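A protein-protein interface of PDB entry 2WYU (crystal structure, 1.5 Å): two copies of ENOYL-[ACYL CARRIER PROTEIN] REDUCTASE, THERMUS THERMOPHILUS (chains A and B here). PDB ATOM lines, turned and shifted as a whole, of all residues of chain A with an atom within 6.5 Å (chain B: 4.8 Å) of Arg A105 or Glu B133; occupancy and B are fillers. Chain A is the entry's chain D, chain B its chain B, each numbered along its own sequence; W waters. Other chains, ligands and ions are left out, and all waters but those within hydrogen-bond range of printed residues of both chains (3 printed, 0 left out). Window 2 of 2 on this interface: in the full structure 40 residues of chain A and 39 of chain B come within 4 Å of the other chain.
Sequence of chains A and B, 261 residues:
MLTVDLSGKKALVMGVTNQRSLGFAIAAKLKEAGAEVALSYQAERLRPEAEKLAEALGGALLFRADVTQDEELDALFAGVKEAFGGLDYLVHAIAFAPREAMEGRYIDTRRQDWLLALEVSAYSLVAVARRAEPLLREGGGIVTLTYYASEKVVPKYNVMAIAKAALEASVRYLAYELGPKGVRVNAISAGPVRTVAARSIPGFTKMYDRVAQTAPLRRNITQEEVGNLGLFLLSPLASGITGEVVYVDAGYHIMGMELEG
OD2 of Asp A108 is in salt-bridge range of NE of Arg A105, 2.9 Å away. The backbone carbonyl oxygen of Tyr A106 sits at hydrogen-bond distance from the side-chain hydroxyl of Thr A109, at 2.6 Å.
Arg A105 touches two residues of chain B. Of chain A, only Arg A105 (2.9 Å) comes within 4 Å of Glu B133. Printed residues of chain A within 4 Å of Arg B130: Ile A107 (3.3 Å) and Asp A108 (3.6 Å). Of the printed residues of chain B, Ile A107 touches Ala B129 (3.8 Å), Arg B130 (3.3 Å) and Glu B177 (2.7 Å). Printed residues of chain B within 4 Å of Tyr A106: Glu B177. Of the printed residues of chain A, Ala B129 touches Ile A107 (3.8 Å). The nearest printed residue of chain B that does not touch Arg A105 is Arg B130 (5.4 Å). The nearest printed residue of chain A that does not touch Ala B129 is Arg A105 (7.4 Å).
No position is printed for both chains.
Hydrophobic or aromatic side chains of chain A that line the printed part of chain B: Tyr A106 and Ile A107. Of the 11 printed residues of chain B, 4 touch a printed residue of chain A. Printed residues of chain B that touch a printed residue of chain A: Ala B129, Arg B130, Glu B133 and Glu B177. Hydrophobic or aromatic side chains of chain B within 4 Å of the printed part of chain A: Ala B129. Among the printed residues, 7 pairs touch across the chains.
OE1 of Glu B133 is in salt-bridge range of NH2 of Arg A105 (2.9 Å). The side-chain carboxylate (OE2) of Glu B177 is in hydrogen-bond range of the backbone NH (N) of Tyr A106. The side-chain carboxylate (OE1) of Glu B177 lies within hydrogen-bond range of the backbone NH (N) of Ile A107.
OE2 of Glu B177 touches CA of Arg A105, 3.4 Å away. Ile A107 touches Ala B129 (CD1 to O, 3.8 Å). Ile A107 touches Arg B130 (O to CB, 3.3 Å). Arg B130 touches Asp A108.
Water W3 lies within hydrogen-bond range of the backbone carbonyl oxygen (O) of Ile A107, the backbone carbonyl oxygen (O) of Thr A109 and the guanidinium group (NH1) of Arg B130. Water W1 bridges OE2 of Glu B177 (2.8 Å) and OD1 of Asn A158 (3.1 Å). Water W2 bridges O of Glu B177 and NH1 of Arg A105.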
ATOM      1  N   GLU A 100     -34.934  14.678  29.197  1.00  0.00           N
ATOM      2  CA  GLU A 100     -34.048  13.685  28.587  1.00  0.00           C
ATOM      3  C   GLU A 100     -33.464  14.190  27.262  1.00  0.00           C
ATOM      4  O   GLU A 100     -32.299  13.928  26.935  1.00  0.00           O
ATOM      5  CB  GLU A 100     -34.806  12.382  28.334  1.00  0.00           C
ATOM      6  CG  GLU A 100     -35.261  11.635  29.601  1.00  0.00           C
ATOM      7  CD  GLU A 100     -36.485  12.260  30.315  1.00  0.00           C
ATOM      8  OE1 GLU A 100     -37.254  13.068  29.701  1.00  0.00           O
ATOM      9  OE2 GLU A 100     -36.674  11.927  31.530  1.00  0.00           O
ATOM     10  N   ALA A 101     -34.288  14.915  26.507  1.00  0.00           N
ATOM     11  CA  ALA A 101     -33.873  15.485  25.229  1.00  0.00           C
ATOM     12  C   ALA A 101     -32.803  16.561  25.413  1.00  0.00           C
ATOM     13  O   ALA A 101     -31.918  16.730  24.553  1.00  0.00           O
ATOM     14  CB  ALA A 101     -35.118  16.056  24.490  1.00  0.00           C
ATOM     15  N   MET A 102     -32.863  17.279  26.541  1.00  0.00           N
ATOM     16  CA  MET A 102     -31.954  18.389  26.804  1.00  0.00           C
ATOM     17  C   MET A 102     -30.666  17.934  27.502  1.00  0.00           C
ATOM     18  O   MET A 102     -29.724  18.708  27.634  1.00  0.00           O
ATOM     19  CB  MET A 102     -32.655  19.493  27.596  1.00  0.00           C
ATOM     20  CG  MET A 102     -33.876  20.074  26.903  1.00  0.00           C
ATOM     21  SD  MET A 102     -33.505  20.821  25.306  1.00  0.00           S
ATOM     22  CE  MET A 102     -32.746  22.352  25.873  1.00  0.00           C
ATOM     23  N   GLU A 103     -30.642  16.688  27.955  1.00  0.00           N
ATOM     24  CA  GLU A 103     -29.424  16.067  28.458  1.00  0.00           C
ATOM     25  C   GLU A 103     -28.753  15.349  27.282  1.00  0.00           C
ATOM     26  O   GLU A 103     -29.422  14.809  26.406  1.00  0.00           O
ATOM     27  CB  GLU A 103     -29.761  15.076  29.583  1.00  0.00           C
ATOM     28  CG  GLU A 103     -30.307  15.726  30.870  1.00  0.00           C
ATOM     29  CD  GLU A 103     -30.864  14.711  31.906  1.00  0.00           C
ATOM     30  OE1 GLU A 103     -31.414  13.643  31.515  1.00  0.00           O
ATOM     31  OE2 GLU A 103     -30.769  15.003  33.125  1.00  0.00           O
ATOM     32  N   GLY A 104     -27.436  15.368  27.235  1.00  0.00           N
ATOM     33  CA  GLY A 104     -26.723  14.645  26.178  1.00  0.00           C
ATOM     34  C   GLY A 104     -26.792  15.300  24.804  1.00  0.00           C
ATOM     35  O   GLY A 104     -26.747  16.538  24.692  1.00  0.00           O
ATOM     36  N   ARG A 105     -26.881  14.455  23.767  1.00  0.00           N
ATOM     37  CA  ARG A 105     -26.665  14.895  22.374  1.00  0.00           C
ATOM     38  C   ARG A 105     -27.955  14.986  21.610  1.00  0.00           C
ATOM     39  O   ARG A 105     -28.898  14.227  21.817  1.00  0.00           O
ATOM     40  CB  ARG A 105     -25.734  13.933  21.634  1.00  0.00           C
ATOM     41  CG  ARG A 105     -24.408  13.651  22.368  1.00  0.00           C
ATOM     42  CD  ARG A 105     -23.464  12.911  21.461  1.00  0.00           C
ATOM     43  NE  ARG A 105     -24.019  11.612  21.083  1.00  0.00           N
ATOM     44  CZ  ARG A 105     -23.568  10.855  20.083  1.00  0.00           C
ATOM     45  NH1 ARG A 105     -22.572  11.271  19.316  1.00  0.00           N
ATOM     46  NH2 ARG A 105     -24.151   9.681  19.819  1.00  0.00           N
ATOM     47  N   TYR A 106     -27.991  15.930  20.683  1.00  0.00           N
ATOM     48  CA  TYR A 106     -29.127  16.034  19.797  1.00  0.00           C
ATOM     49  C   TYR A 106     -29.364  14.757  18.957  1.00  0.00           C
ATOM     50  O   TYR A 106     -30.479  14.326  18.803  1.00  0.00           O
ATOM     51  CB  TYR A 106     -28.983  17.272  18.876  1.00  0.00           C
ATOM     52  CG  TYR A 106     -30.106  17.382  17.874  1.00  0.00           C
ATOM     53  CD1 TYR A 106     -31.411  17.585  18.285  1.00  0.00           C
ATOM     54  CD2 TYR A 106     -29.861  17.238  16.494  1.00  0.00           C
ATOM     55  CE1 TYR A 106     -32.433  17.649  17.378  1.00  0.00           C
ATOM     56  CE2 TYR A 106     -30.903  17.300  15.558  1.00  0.00           C
ATOM     57  CZ  TYR A 106     -32.186  17.490  16.008  1.00  0.00           C
ATOM     58  OH  TYR A 106     -33.279  17.546  15.129  1.00  0.00           O
ATOM     59  N   ILE A 107     -28.291  14.149  18.462  1.00  0.00           N
ATOM     60  CA  ILE A 107     -28.398  12.946  17.634  1.00  0.00           C
ATOM     61  C   ILE A 107     -29.036  11.782  18.407  1.00  0.00           C
ATOM     62  O   ILE A 107     -29.542  10.842  17.796  1.00  0.00           O
ATOM     63  CB  ILE A 107     -27.029  12.558  17.066  1.00  0.00           C
ATOM     64  CG1 ILE A 107     -27.137  11.496  15.987  1.00  0.00           C
ATOM     65  CG2 ILE A 107     -26.063  12.080  18.206  1.00  0.00           C
ATOM     66  CD1 ILE A 107     -25.849  11.219  15.228  1.00  0.00           C
ATOM     67  N   ASP A 108     -28.985  11.841  19.743  1.00  0.00           N
ATOM     68  CA  ASP A 108     -29.579  10.775  20.585  1.00  0.00           C
ATOM     69  C   ASP A 108     -31.016  11.066  21.020  1.00  0.00           C
ATOM     70  O   ASP A 108     -31.595  10.325  21.831  1.00  0.00           O
ATOM     71  CB  ASP A 108     -28.697  10.558  21.816  1.00  0.00           C
ATOM     72  CG  ASP A 108     -27.345  10.002  21.479  1.00  0.00           C
ATOM     73  OD1 ASP A 108     -27.230   9.238  20.501  1.00  0.00           O
ATOM     74  OD2 ASP A 108     -26.378  10.333  22.208  1.00  0.00           O
ATOM     75  N   THR A 109     -31.630  12.130  20.487  1.00  0.00           N
ATOM     76  CA  THR A 109     -32.993  12.493  20.874  1.00  0.00           C
ATOM     77  C   THR A 109     -33.983  11.384  20.512  1.00  0.00           C
ATOM     78  O   THR A 109     -34.068  10.970  19.339  1.00  0.00           O
ATOM     79  CB  THR A 109     -33.472  13.806  20.185  1.00  0.00           C
ATOM     80  OG1 THR A 109     -32.477  14.830  20.358  1.00  0.00           O
ATOM     81  CG2 THR A 109     -34.837  14.254  20.779  1.00  0.00           C
ATOM     82  N   ASN A 158     -29.864  21.631  21.883  1.00  0.00           N
ATOM     83  CA  ASN A 158     -30.408  20.407  21.259  1.00  0.00           C
ATOM     84  C   ASN A 158     -31.731  20.657  20.531  1.00  0.00           C
ATOM     85  O   ASN A 158     -31.819  21.598  19.728  1.00  0.00           O
ATOM     86  CB  ASN A 158     -30.517  19.302  22.335  1.00  0.00           C
ATOM     87  CG  ASN A 158     -29.170  18.869  22.862  1.00  0.00           C
ATOM     88  OD1 ASN A 158     -28.141  19.342  22.412  1.00  0.00           O
ATOM     89  ND2 ASN A 158     -29.177  17.926  23.812  1.00  0.00           N
ATOM     90  N   ALA B 129     -29.213   9.118  11.171  1.00  0.00           N
ATOM     91  CA  ALA B 129     -27.866   9.530  11.533  1.00  0.00           C
ATOM     92  C   ALA B 129     -27.400   8.807  12.763  1.00  0.00           C
ATOM     93  O   ALA B 129     -26.251   8.364  12.824  1.00  0.00           O
ATOM     94  CB  ALA B 129     -27.798  11.069  11.769  1.00  0.00           C
ATOM     95  N   ARG B 130     -28.265   8.703  13.760  1.00  0.00           N
ATOM     96  CA  ARG B 130     -27.862   8.054  15.000  1.00  0.00           C
ATOM     97  C   ARG B 130     -27.472   6.601  14.744  1.00  0.00           C
ATOM     98  O   ARG B 130     -26.488   6.125  15.298  1.00  0.00           O
ATOM     99  CB  ARG B 130     -28.973   8.090  16.028  1.00  0.00           C
ATOM    100  CG  ARG B 130     -28.456   7.626  17.365  1.00  0.00           C
ATOM    101  CD  ARG B 130     -29.518   7.463  18.350  1.00  0.00           C
ATOM    102  NE  ARG B 130     -30.144   6.156  18.215  1.00  0.00           N
ATOM    103  CZ  ARG B 130     -31.449   5.938  18.193  1.00  0.00           C
ATOM    104  NH1 ARG B 130     -32.326   6.945  18.318  1.00  0.00           N
ATOM    105  NH2 ARG B 130     -31.871   4.677  18.097  1.00  0.00           N
ATOM    106  N   ARG B 131     -28.271   5.925  13.941  1.00  0.00           N
ATOM    107  CA  ARG B 131     -28.032   4.506  13.645  1.00  0.00           C
ATOM    108  C   ARG B 131     -26.856   4.321  12.712  1.00  0.00           C
ATOM    109  O   ARG B 131     -26.132   3.296  12.804  1.00  0.00           O
ATOM    110  CB  ARG B 131     -29.285   3.865  13.122  1.00  0.00           C
ATOM    111  CG  ARG B 131     -30.372   3.825  14.175  1.00  0.00           C
ATOM    112  CD  ARG B 131     -31.695   3.471  13.621  1.00  0.00           C
ATOM    113  NE  ARG B 131     -32.656   3.233  14.676  1.00  0.00           N
ATOM    114  CZ  ARG B 131     -33.329   4.178  15.324  1.00  0.00           C
ATOM    115  NH1 ARG B 131     -33.152   5.475  15.035  1.00  0.00           N
ATOM    116  NH2 ARG B 131     -34.206   3.833  16.271  1.00  0.00           N
ATOM    117  N   ALA B 132     -26.648   5.270  11.801  1.00  0.00           N
ATOM    118  CA  ALA B 132     -25.500   5.234  10.896  1.00  0.00           C
ATOM    119  C   ALA B 132     -24.168   5.501  11.623  1.00  0.00           C
ATOM    120  O   ALA B 132     -23.132   5.009  11.175  1.00  0.00           O
ATOM    121  CB  ALA B 132     -25.729   6.223   9.702  1.00  0.00           C
ATOM    122  N   GLU B 133     -24.206   6.284  12.708  1.00  0.00           N
ATOM    123  CA  GLU B 133     -23.003   6.755  13.416  1.00  0.00           C
ATOM    124  C   GLU B 133     -21.953   5.660  13.690  1.00  0.00           C
ATOM    125  O   GLU B 133     -20.812   5.833  13.330  1.00  0.00           O
ATOM    126  CB  GLU B 133     -23.357   7.487  14.711  1.00  0.00           C
ATOM    127  CG  GLU B 133     -22.147   8.007  15.455  1.00  0.00           C
ATOM    128  CD  GLU B 133     -22.474   8.757  16.717  1.00  0.00           C
ATOM    129  OE1 GLU B 133     -23.577   8.563  17.252  1.00  0.00           O
ATOM    130  OE2 GLU B 133     -21.610   9.539  17.167  1.00  0.00           O
ATOM    131  N   PRO B 134     -22.347   4.544  14.335  1.00  0.00           N
ATOM    132  CA  PRO B 134     -21.326   3.514  14.582  1.00  0.00           C
ATOM    133  C   PRO B 134     -20.778   2.804  13.334  1.00  0.00           C
ATOM    134  O   PRO B 134     -19.685   2.216  13.385  1.00  0.00           O
ATOM    135  CB  PRO B 134     -22.046   2.530  15.509  1.00  0.00           C
ATOM    136  CG  PRO B 134     -23.458   2.748  15.291  1.00  0.00           C
ATOM    137  CD  PRO B 134     -23.611   4.215  14.997  1.00  0.00           C
ATOM    138  N   LEU B 135     -21.507   2.858  12.231  1.00  0.00           N
ATOM    139  CA  LEU B 135     -21.045   2.292  10.967  1.00  0.00           C
ATOM    140  C   LEU B 135     -20.230   3.226  10.088  1.00  0.00           C
ATOM    141  O   LEU B 135     -19.462   2.781   9.260  1.00  0.00           O
ATOM    142  CB  LEU B 135     -22.242   1.845  10.140  1.00  0.00           C
ATOM    143  CG  LEU B 135     -23.138   0.767  10.728  1.00  0.00           C
ATOM    144  CD1 LEU B 135     -24.197   0.429   9.720  1.00  0.00           C
ATOM    145  CD2 LEU B 135     -22.317  -0.451  11.106  1.00  0.00           C
ATOM    146  N   LEU B 136     -20.455   4.530  10.213  1.00  0.00           N
ATOM    147  CA  LEU B 136     -19.813   5.492   9.331  1.00  0.00           C
ATOM    148  C   LEU B 136     -18.299   5.572   9.521  1.00  0.00           C
ATOM    149  O   LEU B 136     -17.820   5.745  10.628  1.00  0.00           O
ATOM    150  CB  LEU B 136     -20.465   6.886   9.506  1.00  0.00           C
ATOM    151  CG  LEU B 136     -21.843   7.043   8.846  1.00  0.00           C
ATOM    152  CD1 LEU B 136     -22.671   8.264   9.398  1.00  0.00           C
ATOM    153  CD2 LEU B 136     -21.734   7.105   7.316  1.00  0.00           C
ATOM    154  N   GLU B 177     -21.965  17.227  15.974  1.00  0.00           N
ATOM    155  CA  GLU B 177     -21.840  16.000  16.789  1.00  0.00           C
ATOM    156  C   GLU B 177     -21.096  14.863  16.084  1.00  0.00           C
ATOM    157  O   GLU B 177     -20.473  14.027  16.763  1.00  0.00           O
ATOM    158  CB  GLU B 177     -23.216  15.584  17.308  1.00  0.00           C
ATOM    159  CG  GLU B 177     -23.830  16.639  18.197  1.00  0.00           C
ATOM    160  CD  GLU B 177     -25.183  16.299  18.784  1.00  0.00           C
ATOM    161  OE1 GLU B 177     -25.895  15.434  18.240  1.00  0.00           O
ATOM    162  OE2 GLU B 177     -25.592  16.911  19.804  1.00  0.00           O
ATOM    163  N   LEU B 178     -21.130  14.814  14.755  1.00  0.00           N
ATOM    164  CA  LEU B 178     -20.437  13.795  13.958  1.00  0.00           C
ATOM    165  C   LEU B 178     -19.029  14.218  13.522  1.00  0.00           C
ATOM    166  O   LEU B 178     -18.190  13.384  13.200  1.00  0.00           O
ATOM    167  CB  LEU B 178     -21.287  13.407  12.733  1.00  0.00           C
ATOM    168  CG  LEU B 178     -22.565  12.623  13.072  1.00  0.00           C
ATOM    169  CD1 LEU B 178     -23.490  12.398  11.927  1.00  0.00           C
ATOM    170  CD2 LEU B 178     -22.164  11.208  13.637  1.00  0.00           C
ATOM    171  N   LYS B 181     -15.647  12.407  14.574  1.00  0.00           N
ATOM    172  CA  LYS B 181     -15.379  11.162  13.851  1.00  0.00           C
ATOM    173  C   LYS B 181     -14.889  11.362  12.420  1.00  0.00           C
ATOM    174  O   LYS B 181     -14.686  10.380  11.722  1.00  0.00           O
ATOM    175  CB  LYS B 181     -16.648  10.315  13.734  1.00  0.00           C
ATOM    176  CG  LYS B 181     -17.097   9.535  14.950  1.00  0.00           C
ATOM    177  CD  LYS B 181     -18.328   8.650  14.611  1.00  0.00           C
ATOM    178  CE  LYS B 181     -17.945   7.219  14.191  1.00  0.00           C
ATOM    179  NZ  LYS B 181     -17.961   6.289  15.370  1.00  0.00           N
HETATM  180  O   HOH W   1     -25.361  19.402  21.037  1.00  0.00           O
HETATM  181  O   HOH W   2     -20.770  13.572  19.524  1.00  0.00           O
HETATM  182  O   HOH W   3     -32.071   9.725  17.794  1.00  0.00           O
